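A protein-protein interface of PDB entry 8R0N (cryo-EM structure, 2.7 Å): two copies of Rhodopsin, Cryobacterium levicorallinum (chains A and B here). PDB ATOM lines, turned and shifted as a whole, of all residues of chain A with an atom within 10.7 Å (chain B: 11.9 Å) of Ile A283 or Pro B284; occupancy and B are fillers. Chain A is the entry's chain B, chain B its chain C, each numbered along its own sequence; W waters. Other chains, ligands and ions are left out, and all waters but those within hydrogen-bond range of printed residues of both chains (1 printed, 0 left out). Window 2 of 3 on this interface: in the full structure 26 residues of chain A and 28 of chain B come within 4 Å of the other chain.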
ATOM      1  N   VAL A 260     -24.805  -9.212 -32.864  1.00  0.00           N
ATOM      2  CA  VAL A 260     -24.599 -10.365 -32.018  1.00  0.00           C
ATOM      3  C   VAL A 260     -25.850 -11.211 -32.035  1.00  0.00           C
ATOM      4  O   VAL A 260     -25.783 -12.415 -32.222  1.00  0.00           O
ATOM      5  CB  VAL A 260     -24.228  -9.949 -30.609  1.00  0.00           C
ATOM      6  CG1 VAL A 260     -24.290 -11.131 -29.694  1.00  0.00           C
ATOM      7  CG2 VAL A 260     -22.863  -9.325 -30.532  1.00  0.00           C
ATOM      8  N   GLY A 263     -26.200 -13.009 -35.446  1.00  0.00           N
ATOM      9  CA  GLY A 263     -25.156 -13.929 -35.827  1.00  0.00           C
ATOM     10  C   GLY A 263     -24.137 -13.295 -36.763  1.00  0.00           C
ATOM     11  O   GLY A 263     -23.175 -13.939 -37.190  1.00  0.00           O
ATOM     12  N   ASP A 265     -21.983 -11.249 -35.924  1.00  0.00           N
ATOM     13  CA  ASP A 265     -20.704 -11.251 -35.234  1.00  0.00           C
ATOM     14  C   ASP A 265     -20.899 -11.706 -33.786  1.00  0.00           C
ATOM     15  O   ASP A 265     -21.998 -12.086 -33.425  1.00  0.00           O
ATOM     16  CB  ASP A 265     -20.027  -9.892 -35.367  1.00  0.00           C
ATOM     17  CG  ASP A 265     -18.500  -9.904 -35.397  1.00  0.00           C
ATOM     18  OD1 ASP A 265     -17.883 -10.938 -35.022  1.00  0.00           O
ATOM     19  OD2 ASP A 265     -17.923  -8.846 -35.789  1.00  0.00           O
ATOM     20  N   ILE A 266     -19.825 -11.818 -33.008  1.00  0.00           N
ATOM     21  CA  ILE A 266     -19.903 -12.243 -31.621  1.00  0.00           C
ATOM     22  C   ILE A 266     -19.173 -11.194 -30.808  1.00  0.00           C
ATOM     23  O   ILE A 266     -18.301 -10.542 -31.348  1.00  0.00           O
ATOM     24  CB  ILE A 266     -19.303 -13.652 -31.403  1.00  0.00           C
ATOM     25  CG1 ILE A 266     -17.789 -13.723 -31.523  1.00  0.00           C
ATOM     26  CG2 ILE A 266     -19.905 -14.654 -32.354  1.00  0.00           C
ATOM     27  CD1 ILE A 266     -17.096 -13.691 -30.208  1.00  0.00           C
ATOM     28  N   HIS A 267     -19.546 -10.985 -29.546  1.00  0.00           N
ATOM     29  CA  HIS A 267     -18.901  -9.943 -28.762  1.00  0.00           C
ATOM     30  C   HIS A 267     -18.462 -10.595 -27.483  1.00  0.00           C
ATOM     31  O   HIS A 267     -19.123 -11.508 -27.020  1.00  0.00           O
ATOM     32  CB  HIS A 267     -19.832  -8.740 -28.568  1.00  0.00           C
ATOM     33  CG  HIS A 267     -19.144  -7.475 -28.191  1.00  0.00           C
ATOM     34  ND1 HIS A 267     -19.248  -6.889 -26.946  1.00  0.00           N
ATOM     35  CD2 HIS A 267     -18.273  -6.717 -28.877  1.00  0.00           C
ATOM     36  CE1 HIS A 267     -18.441  -5.828 -26.900  1.00  0.00           C
ATOM     37  NE2 HIS A 267     -17.849  -5.691 -28.065  1.00  0.00           N
ATOM     38  N   THR A 268     -17.315 -10.185 -26.962  1.00  0.00           N
ATOM     39  CA  THR A 268     -16.735 -10.875 -25.819  1.00  0.00           C
ATOM     40  C   THR A 268     -17.496 -10.576 -24.530  1.00  0.00           C
ATOM     41  O   THR A 268     -17.490 -11.408 -23.633  1.00  0.00           O
ATOM     42  CB  THR A 268     -15.273 -10.467 -25.643  1.00  0.00           C
ATOM     43  OG1 THR A 268     -15.221  -9.038 -25.681  1.00  0.00           O
ATOM     44  CG2 THR A 268     -14.393 -11.054 -26.727  1.00  0.00           C
ATOM     45  N   GLU A 269     -18.089  -9.392 -24.406  1.00  0.00           N
ATOM     46  CA  GLU A 269     -18.779  -9.033 -23.182  1.00  0.00           C
ATOM     47  C   GLU A 269     -20.237  -8.751 -23.516  1.00  0.00           C
ATOM     48  O   GLU A 269     -20.544  -8.472 -24.676  1.00  0.00           O
ATOM     49  CB  GLU A 269     -18.093  -7.844 -22.519  1.00  0.00           C
ATOM     50  CG  GLU A 269     -18.105  -6.613 -23.382  1.00  0.00           C
ATOM     51  CD  GLU A 269     -18.083  -5.278 -22.651  1.00  0.00           C
ATOM     52  OE1 GLU A 269     -17.043  -4.997 -22.004  1.00  0.00           O
ATOM     53  OE2 GLU A 269     -19.111  -4.507 -22.775  1.00  0.00           O
ATOM     54  N   ALA A 270     -21.123  -8.822 -22.513  1.00  0.00           N
ATOM     55  CA  ALA A 270     -22.508  -8.441 -22.729  1.00  0.00           C
ATOM     56  C   ALA A 270     -22.594  -6.933 -22.897  1.00  0.00           C
ATOM     57  O   ALA A 270     -21.719  -6.201 -22.426  1.00  0.00           O
ATOM     58  CB  ALA A 270     -23.392  -8.843 -21.616  1.00  0.00           C
ATOM     59  N   LYS A 277     -29.844  -5.328 -20.610  1.00  0.00           N
ATOM     60  CA  LYS A 277     -28.916  -6.160 -21.353  1.00  0.00           C
ATOM     61  C   LYS A 277     -29.454  -6.263 -22.761  1.00  0.00           C
ATOM     62  O   LYS A 277     -30.642  -6.530 -22.923  1.00  0.00           O
ATOM     63  CB  LYS A 277     -28.827  -7.547 -20.731  1.00  0.00           C
ATOM     64  CG  LYS A 277     -27.544  -8.308 -20.976  1.00  0.00           C
ATOM     65  CD  LYS A 277     -27.587  -9.693 -20.422  1.00  0.00           C
ATOM     66  CE  LYS A 277     -26.235 -10.339 -20.513  1.00  0.00           C
ATOM     67  NZ  LYS A 277     -26.297 -11.743 -20.041  1.00  0.00           N
ATOM     68  N   SER A 279     -27.382  -7.740 -25.374  1.00  0.00           N
ATOM     69  CA  SER A 279     -26.802  -8.937 -25.960  1.00  0.00           C
ATOM     70  C   SER A 279     -25.946  -9.618 -24.899  1.00  0.00           C
ATOM     71  O   SER A 279     -25.414  -8.939 -24.029  1.00  0.00           O
ATOM     72  CB  SER A 279     -25.946  -8.587 -27.159  1.00  0.00           C
ATOM     73  OG  SER A 279     -24.729  -7.924 -26.748  1.00  0.00           O
ATOM     74  N   ASP A 280     -25.722 -10.937 -25.038  1.00  0.00           N
ATOM     75  CA  ASP A 280     -24.891 -11.705 -24.112  1.00  0.00           C
ATOM     76  C   ASP A 280     -23.466 -11.813 -24.637  1.00  0.00           C
ATOM     77  O   ASP A 280     -23.241 -11.587 -25.825  1.00  0.00           O
ATOM     78  CB  ASP A 280     -25.460 -13.093 -23.933  1.00  0.00           C
ATOM     79  CG  ASP A 280     -26.875 -13.061 -23.409  1.00  0.00           C
ATOM     80  OD1 ASP A 280     -27.347 -11.949 -23.031  1.00  0.00           O
ATOM     81  OD2 ASP A 280     -27.520 -14.140 -23.415  1.00  0.00           O
ATOM     82  N   ALA A 281     -22.519 -12.158 -23.750  1.00  0.00           N
ATOM     83  CA  ALA A 281     -21.144 -12.464 -24.139  1.00  0.00           C
ATOM     84  C   ALA A 281     -21.082 -13.820 -24.843  1.00  0.00           C
ATOM     85  O   ALA A 281     -21.871 -14.714 -24.525  1.00  0.00           O
ATOM     86  CB  ALA A 281     -20.252 -12.468 -22.937  1.00  0.00           C
ATOM     87  N   GLY A 282     -20.138 -13.942 -25.794  1.00  0.00           N
ATOM     88  CA  GLY A 282     -19.986 -15.139 -26.612  1.00  0.00           C
ATOM     89  C   GLY A 282     -18.520 -15.461 -26.909  1.00  0.00           C
ATOM     90  O   GLY A 282     -17.661 -14.577 -26.835  1.00  0.00           O
ATOM     91  N   ILE A 283     -18.244 -16.734 -27.241  1.00  0.00           N
ATOM     92  CA  ILE A 283     -16.882 -17.185 -27.526  1.00  0.00           C
ATOM     93  C   ILE A 283     -16.754 -17.458 -29.025  1.00  0.00           C
ATOM     94  O   ILE A 283     -17.661 -18.026 -29.641  1.00  0.00           O
ATOM     95  CB  ILE A 283     -16.460 -18.421 -26.700  1.00  0.00           C
ATOM     96  CG1 ILE A 283     -17.562 -19.489 -26.687  1.00  0.00           C
ATOM     97  CG2 ILE A 283     -16.030 -18.017 -25.296  1.00  0.00           C
ATOM     98  CD1 ILE A 283     -17.240 -20.733 -25.894  1.00  0.00           C
ATOM     99  N   PRO A 284     -15.615 -17.053 -29.647  1.00  0.00           N
ATOM    100  CA  PRO A 284     -15.399 -17.264 -31.078  1.00  0.00           C
ATOM    101  C   PRO A 284     -15.588 -18.733 -31.416  1.00  0.00           C
ATOM    102  O   PRO A 284     -14.874 -19.572 -30.881  1.00  0.00           O
ATOM    103  CB  PRO A 284     -13.948 -16.834 -31.301  1.00  0.00           C
ATOM    104  CG  PRO A 284     -13.675 -15.832 -30.188  1.00  0.00           C
ATOM    105  CD  PRO A 284     -14.491 -16.336 -29.010  1.00  0.00           C
ATOM    106  N   THR A 285     -16.575 -19.031 -32.265  1.00  0.00           N
ATOM    107  CA  THR A 285     -16.885 -20.405 -32.644  1.00  0.00           C
ATOM    108  C   THR A 285     -16.882 -21.309 -31.400  1.00  0.00           C
ATOM    109  O   THR A 285     -17.083 -22.530 -31.576  1.00  0.00           O
ATOM    110  CB  THR A 285     -15.921 -20.928 -33.726  1.00  0.00           C
ATOM    111  N   ALA B  48     -19.773  -4.987 -16.833  1.00  0.00           N
ATOM    112  CA  ALA B  48     -20.088  -3.934 -17.769  1.00  0.00           C
ATOM    113  C   ALA B  48     -21.399  -3.264 -17.377  1.00  0.00           C
ATOM    114  O   ALA B  48     -21.596  -2.107 -17.714  1.00  0.00           O
ATOM    115  CB  ALA B  48     -20.153  -4.535 -19.143  1.00  0.00           C
ATOM    116  N   VAL B 260     -23.430 -12.759 -11.487  1.00  0.00           N
ATOM    117  CA  VAL B 260     -22.745 -13.955 -11.922  1.00  0.00           C
ATOM    118  C   VAL B 260     -23.407 -15.154 -11.281  1.00  0.00           C
ATOM    119  O   VAL B 260     -23.712 -16.125 -11.954  1.00  0.00           O
ATOM    120  CB  VAL B 260     -21.270 -13.889 -11.587  1.00  0.00           C
ATOM    121  CG1 VAL B 260     -20.641 -15.231 -11.786  1.00  0.00           C
ATOM    122  CG2 VAL B 260     -20.536 -12.860 -12.401  1.00  0.00           C
ATOM    123  N   GLY B 263     -26.857 -15.802 -12.912  1.00  0.00           N
ATOM    124  CA  GLY B 263     -26.883 -16.104 -14.322  1.00  0.00           C
ATOM    125  C   GLY B 263     -27.202 -14.883 -15.173  1.00  0.00           C
ATOM    126  O   GLY B 263     -27.263 -14.958 -16.404  1.00  0.00           O
ATOM    127  N   VAL B 264     -27.417 -13.756 -14.519  1.00  0.00           N
ATOM    128  CA  VAL B 264     -27.672 -12.524 -15.232  1.00  0.00           C
ATOM    129  C   VAL B 264     -26.480 -12.182 -16.128  1.00  0.00           C
ATOM    130  O   VAL B 264     -26.659 -11.506 -17.125  1.00  0.00           O
ATOM    131  CB  VAL B 264     -27.926 -11.396 -14.229  1.00  0.00           C
ATOM    132  CG1 VAL B 264     -28.069 -10.058 -14.914  1.00  0.00           C
ATOM    133  CG2 VAL B 264     -29.128 -11.716 -13.378  1.00  0.00           C
ATOM    134  N   ASP B 265     -25.263 -12.551 -15.739  1.00  0.00           N
ATOM    135  CA  ASP B 265     -24.104 -12.284 -16.568  1.00  0.00           C
ATOM    136  C   ASP B 265     -22.949 -13.203 -16.158  1.00  0.00           C
ATOM    137  O   ASP B 265     -23.144 -14.059 -15.317  1.00  0.00           O
ATOM    138  CB  ASP B 265     -23.751 -10.801 -16.535  1.00  0.00           C
ATOM    139  CG  ASP B 265     -23.133 -10.236 -17.815  1.00  0.00           C
ATOM    140  OD1 ASP B 265     -22.699 -11.046 -18.710  1.00  0.00           O
ATOM    141  OD2 ASP B 265     -23.063  -8.974 -17.911  1.00  0.00           O
ATOM    142  N   ILE B 266     -21.815 -13.140 -16.850  1.00  0.00           N
ATOM    143  CA  ILE B 266     -20.663 -13.967 -16.547  1.00  0.00           C
ATOM    144  C   ILE B 266     -19.484 -13.026 -16.410  1.00  0.00           C
ATOM    145  O   ILE B 266     -19.511 -11.967 -17.005  1.00  0.00           O
ATOM    146  CB  ILE B 266     -20.412 -15.046 -17.628  1.00  0.00           C
ATOM    147  CG1 ILE B 266     -19.900 -14.508 -18.954  1.00  0.00           C
ATOM    148  CG2 ILE B 266     -21.658 -15.853 -17.896  1.00  0.00           C
ATOM    149  CD1 ILE B 266     -18.433 -14.628 -19.108  1.00  0.00           C
ATOM    150  N   HIS B 267     -18.482 -13.367 -15.604  1.00  0.00           N
ATOM    151  CA  HIS B 267     -17.367 -12.454 -15.395  1.00  0.00           C
ATOM    152  C   HIS B 267     -16.126 -13.262 -15.649  1.00  0.00           C
ATOM    153  O   HIS B 267     -16.119 -14.452 -15.378  1.00  0.00           O
ATOM    154  CB  HIS B 267     -17.424 -11.810 -14.002  1.00  0.00           C
ATOM    155  CG  HIS B 267     -16.610 -10.572 -13.855  1.00  0.00           C
ATOM    156  ND1 HIS B 267     -15.463 -10.487 -13.093  1.00  0.00           N
ATOM    157  CD2 HIS B 267     -16.748  -9.368 -14.442  1.00  0.00           C
ATOM    158  CE1 HIS B 267     -14.923  -9.276 -13.256  1.00  0.00           C
ATOM    159  NE2 HIS B 267     -15.697  -8.569 -14.058  1.00  0.00           N
ATOM    160  N   THR B 268     -15.116 -12.639 -16.240  1.00  0.00           N
ATOM    161  CA  THR B 268     -13.946 -13.385 -16.678  1.00  0.00           C
ATOM    162  C   THR B 268     -13.076 -13.814 -15.499  1.00  0.00           C
ATOM    163  O   THR B 268     -12.387 -14.821 -15.608  1.00  0.00           O
ATOM    164  CB  THR B 268     -13.106 -12.536 -17.632  1.00  0.00           C
ATOM    165  OG1 THR B 268     -12.922 -11.256 -17.019  1.00  0.00           O
ATOM    166  CG2 THR B 268     -13.777 -12.375 -18.979  1.00  0.00           C
ATOM    167  N   GLU B 269     -13.051 -13.037 -14.415  1.00  0.00           N
ATOM    168  CA  GLU B 269     -12.211 -13.371 -13.287  1.00  0.00           C
ATOM    169  C   GLU B 269     -13.084 -13.551 -12.056  1.00  0.00           C
ATOM    170  O   GLU B 269     -14.209 -13.058 -12.047  1.00  0.00           O
ATOM    171  CB  GLU B 269     -11.150 -12.299 -13.108  1.00  0.00           C
ATOM    172  CG  GLU B 269     -11.708 -10.960 -12.716  1.00  0.00           C
ATOM    173  CD  GLU B 269     -10.608 -10.039 -12.214  1.00  0.00           C
ATOM    174  OE1 GLU B 269     -10.883  -9.249 -11.274  1.00  0.00           O
ATOM    175  OE2 GLU B 269      -9.472 -10.149 -12.753  1.00  0.00           O
ATOM    176  N   ASP B 280     -17.051 -17.028  -9.032  1.00  0.00           N
ATOM    177  CA  ASP B 280     -15.975 -17.675  -9.780  1.00  0.00           C
ATOM    178  C   ASP B 280     -15.855 -17.076 -11.173  1.00  0.00           C
ATOM    179  O   ASP B 280     -16.793 -16.427 -11.635  1.00  0.00           O
ATOM    180  CB  ASP B 280     -16.242 -19.157  -9.899  1.00  0.00           C
ATOM    181  CG  ASP B 280     -16.362 -19.820  -8.549  1.00  0.00           C
ATOM    182  OD1 ASP B 280     -16.071 -19.139  -7.522  1.00  0.00           O
ATOM    183  OD2 ASP B 280     -16.778 -21.004  -8.519  1.00  0.00           O
ATOM    184  N   ALA B 281     -14.705 -17.301 -11.832  1.00  0.00           N
ATOM    185  CA  ALA B 281     -14.517 -16.941 -13.235  1.00  0.00           C
ATOM    186  C   ALA B 281     -15.308 -17.882 -14.145  1.00  0.00           C
ATOM    187  O   ALA B 281     -15.485 -19.055 -13.807  1.00  0.00           O
ATOM    188  CB  ALA B 281     -13.066 -16.988 -13.590  1.00  0.00           C
ATOM    189  N   GLY B 282     -15.776 -17.341 -15.285  1.00  0.00           N
ATOM    190  CA  GLY B 282     -16.615 -18.076 -16.223  1.00  0.00           C
ATOM    191  C   GLY B 282     -16.320 -17.719 -17.682  1.00  0.00           C
ATOM    192  O   GLY B 282     -15.773 -16.648 -17.959  1.00  0.00           O
ATOM    193  N   ILE B 283     -16.682 -18.622 -18.607  1.00  0.00           N
ATOM    194  CA  ILE B 283     -16.450 -18.418 -20.035  1.00  0.00           C
ATOM    195  C   ILE B 283     -17.796 -18.190 -20.724  1.00  0.00           C
ATOM    196  O   ILE B 283     -18.785 -18.866 -20.415  1.00  0.00           O
ATOM    197  CB  ILE B 283     -15.679 -19.584 -20.702  1.00  0.00           C
ATOM    198  CG1 ILE B 283     -16.233 -20.947 -20.273  1.00  0.00           C
ATOM    199  CG2 ILE B 283     -14.185 -19.471 -20.443  1.00  0.00           C
ATOM    200  CD1 ILE B 283     -15.568 -22.131 -20.927  1.00  0.00           C
ATOM    201  N   PRO B 284     -17.860 -17.240 -21.694  1.00  0.00           N
ATOM    202  CA  PRO B 284     -19.094 -16.960 -22.424  1.00  0.00           C
ATOM    203  C   PRO B 284     -19.643 -18.246 -23.025  1.00  0.00           C
ATOM    204  O   PRO B 284     -18.964 -18.880 -23.825  1.00  0.00           O
ATOM    205  CB  PRO B 284     -18.658 -15.998 -23.531  1.00  0.00           C
ATOM    206  CG  PRO B 284     -17.430 -15.305 -22.966  1.00  0.00           C
ATOM    207  CD  PRO B 284     -16.748 -16.369 -22.124  1.00  0.00           C
ATOM    208  N   THR B 285     -20.848 -18.640 -22.600  1.00  0.00           N
ATOM    209  CA  THR B 285     -21.480 -19.862 -23.085  1.00  0.00           C
ATOM    210  C   THR B 285     -20.456 -21.011 -23.106  1.00  0.00           C
ATOM    211  O   THR B 285     -20.821 -22.102 -23.608  1.00  0.00           O
ATOM    212  CB  THR B 285     -22.140 -19.647 -24.461  1.00  0.00           C
HETATM  213  O   HOH W   1     -20.440  -9.992 -19.789  1.00  0.00           O
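Thr A268 touches Pro B284, but with the chains exchanged Pro A284 does not touch Thr B268 (10.8 Å).
Ala A281 touches Pro B284, but with the chains exchanged Pro A284 does not touch Ala B281 (15.0 Å).
Gly A282 touches Pro B284, but with the chains exchanged Pro A284 does not touch Gly B282 (11.1 Å).
Ile A283 touches Pro B284, but with the chains exchanged Pro A284 does not touch Ile B283 (9.0 Å).
Positions printed for both chains: 260, 263, 265, 266, 267, 268, 269, 280, 281, 282, 283, 284 and 285.
ND1 of His A267 sits at hydrogen-bond distance from O of Glu A269 (3.1 Å).
The backbone carbonyl oxygen of His A267 lies within hydrogen-bond range of the backbone NH of Gly A282 (2.9 Å).
The side-chain amino group of Lys A277 is in salt-bridge range of the side-chain carboxylate of Asp A280, 3.2 Å away.
Printed residues of chain A that touch a printed residue of chain B: Thr A268, Glu A269, Ala A270, Lys A277, Ala A281, Gly A282 and Ile A283.
Hydrophobic or aromatic side chains of chain A that line the printed part of chain B: Ala A270, Ala A281 and Ile A283.
Printed residues of chain B that touch a printed residue of chain A: Ala B48, Val B264, Asp B265 and Pro B284.
Among the printed residues, 8 pairs touch across the chains.
No residue of chain B comes within 4 Å of Ile A266.
Printed residues of chain B within 4 Å of Glu A269: Ala B48 (3.8 Å).
Of chain B, only Pro B284 comes within 4 Å of Gly A282.
Of chain B, only Pro B284 (3.2 Å) comes within 4 Å of Ile A283.
No residue of chain B comes within 4 Å of Pro A284.
No residue of chain B comes within 4 Å of Thr A285.
Printed residues of chain A within 4 Å of Ala B48: Glu A269.
Pro B284 touches just these residues of chain A: Thr A268, Ala A281, Gly A282 and Ile A283.
The nearest residue of chain B that does not touch Ile A283 is Thr B285 (4.3 Å).
The nearest residue of chain A that does not touch Pro B284 is His A267 (5.7 Å).
The nearest printed residue of chain A that does not touch Asp B265 is Ala A281 (5.1 Å).
Among the printed residues, merely in contact across the chains: Ile A283 with Pro B284, Gly A282 with Pro B284, Ala A281 with Pro B284, Ala A270 with Asp B265, Glu A269 with Ala B48 and Thr A268 with Pro B284.
NZ of Lys A277 sits at hydrogen-bond distance from O of Val B264, 2.9 Å away.
The side-chain carboxylate (OD1) of Asp B265 is in salt-bridge range of the side-chain amino group (NZ) of Lys A277, 3.9 Å away.
Water W1 bridges OD1 of Asp B265 and N of Ala A270.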
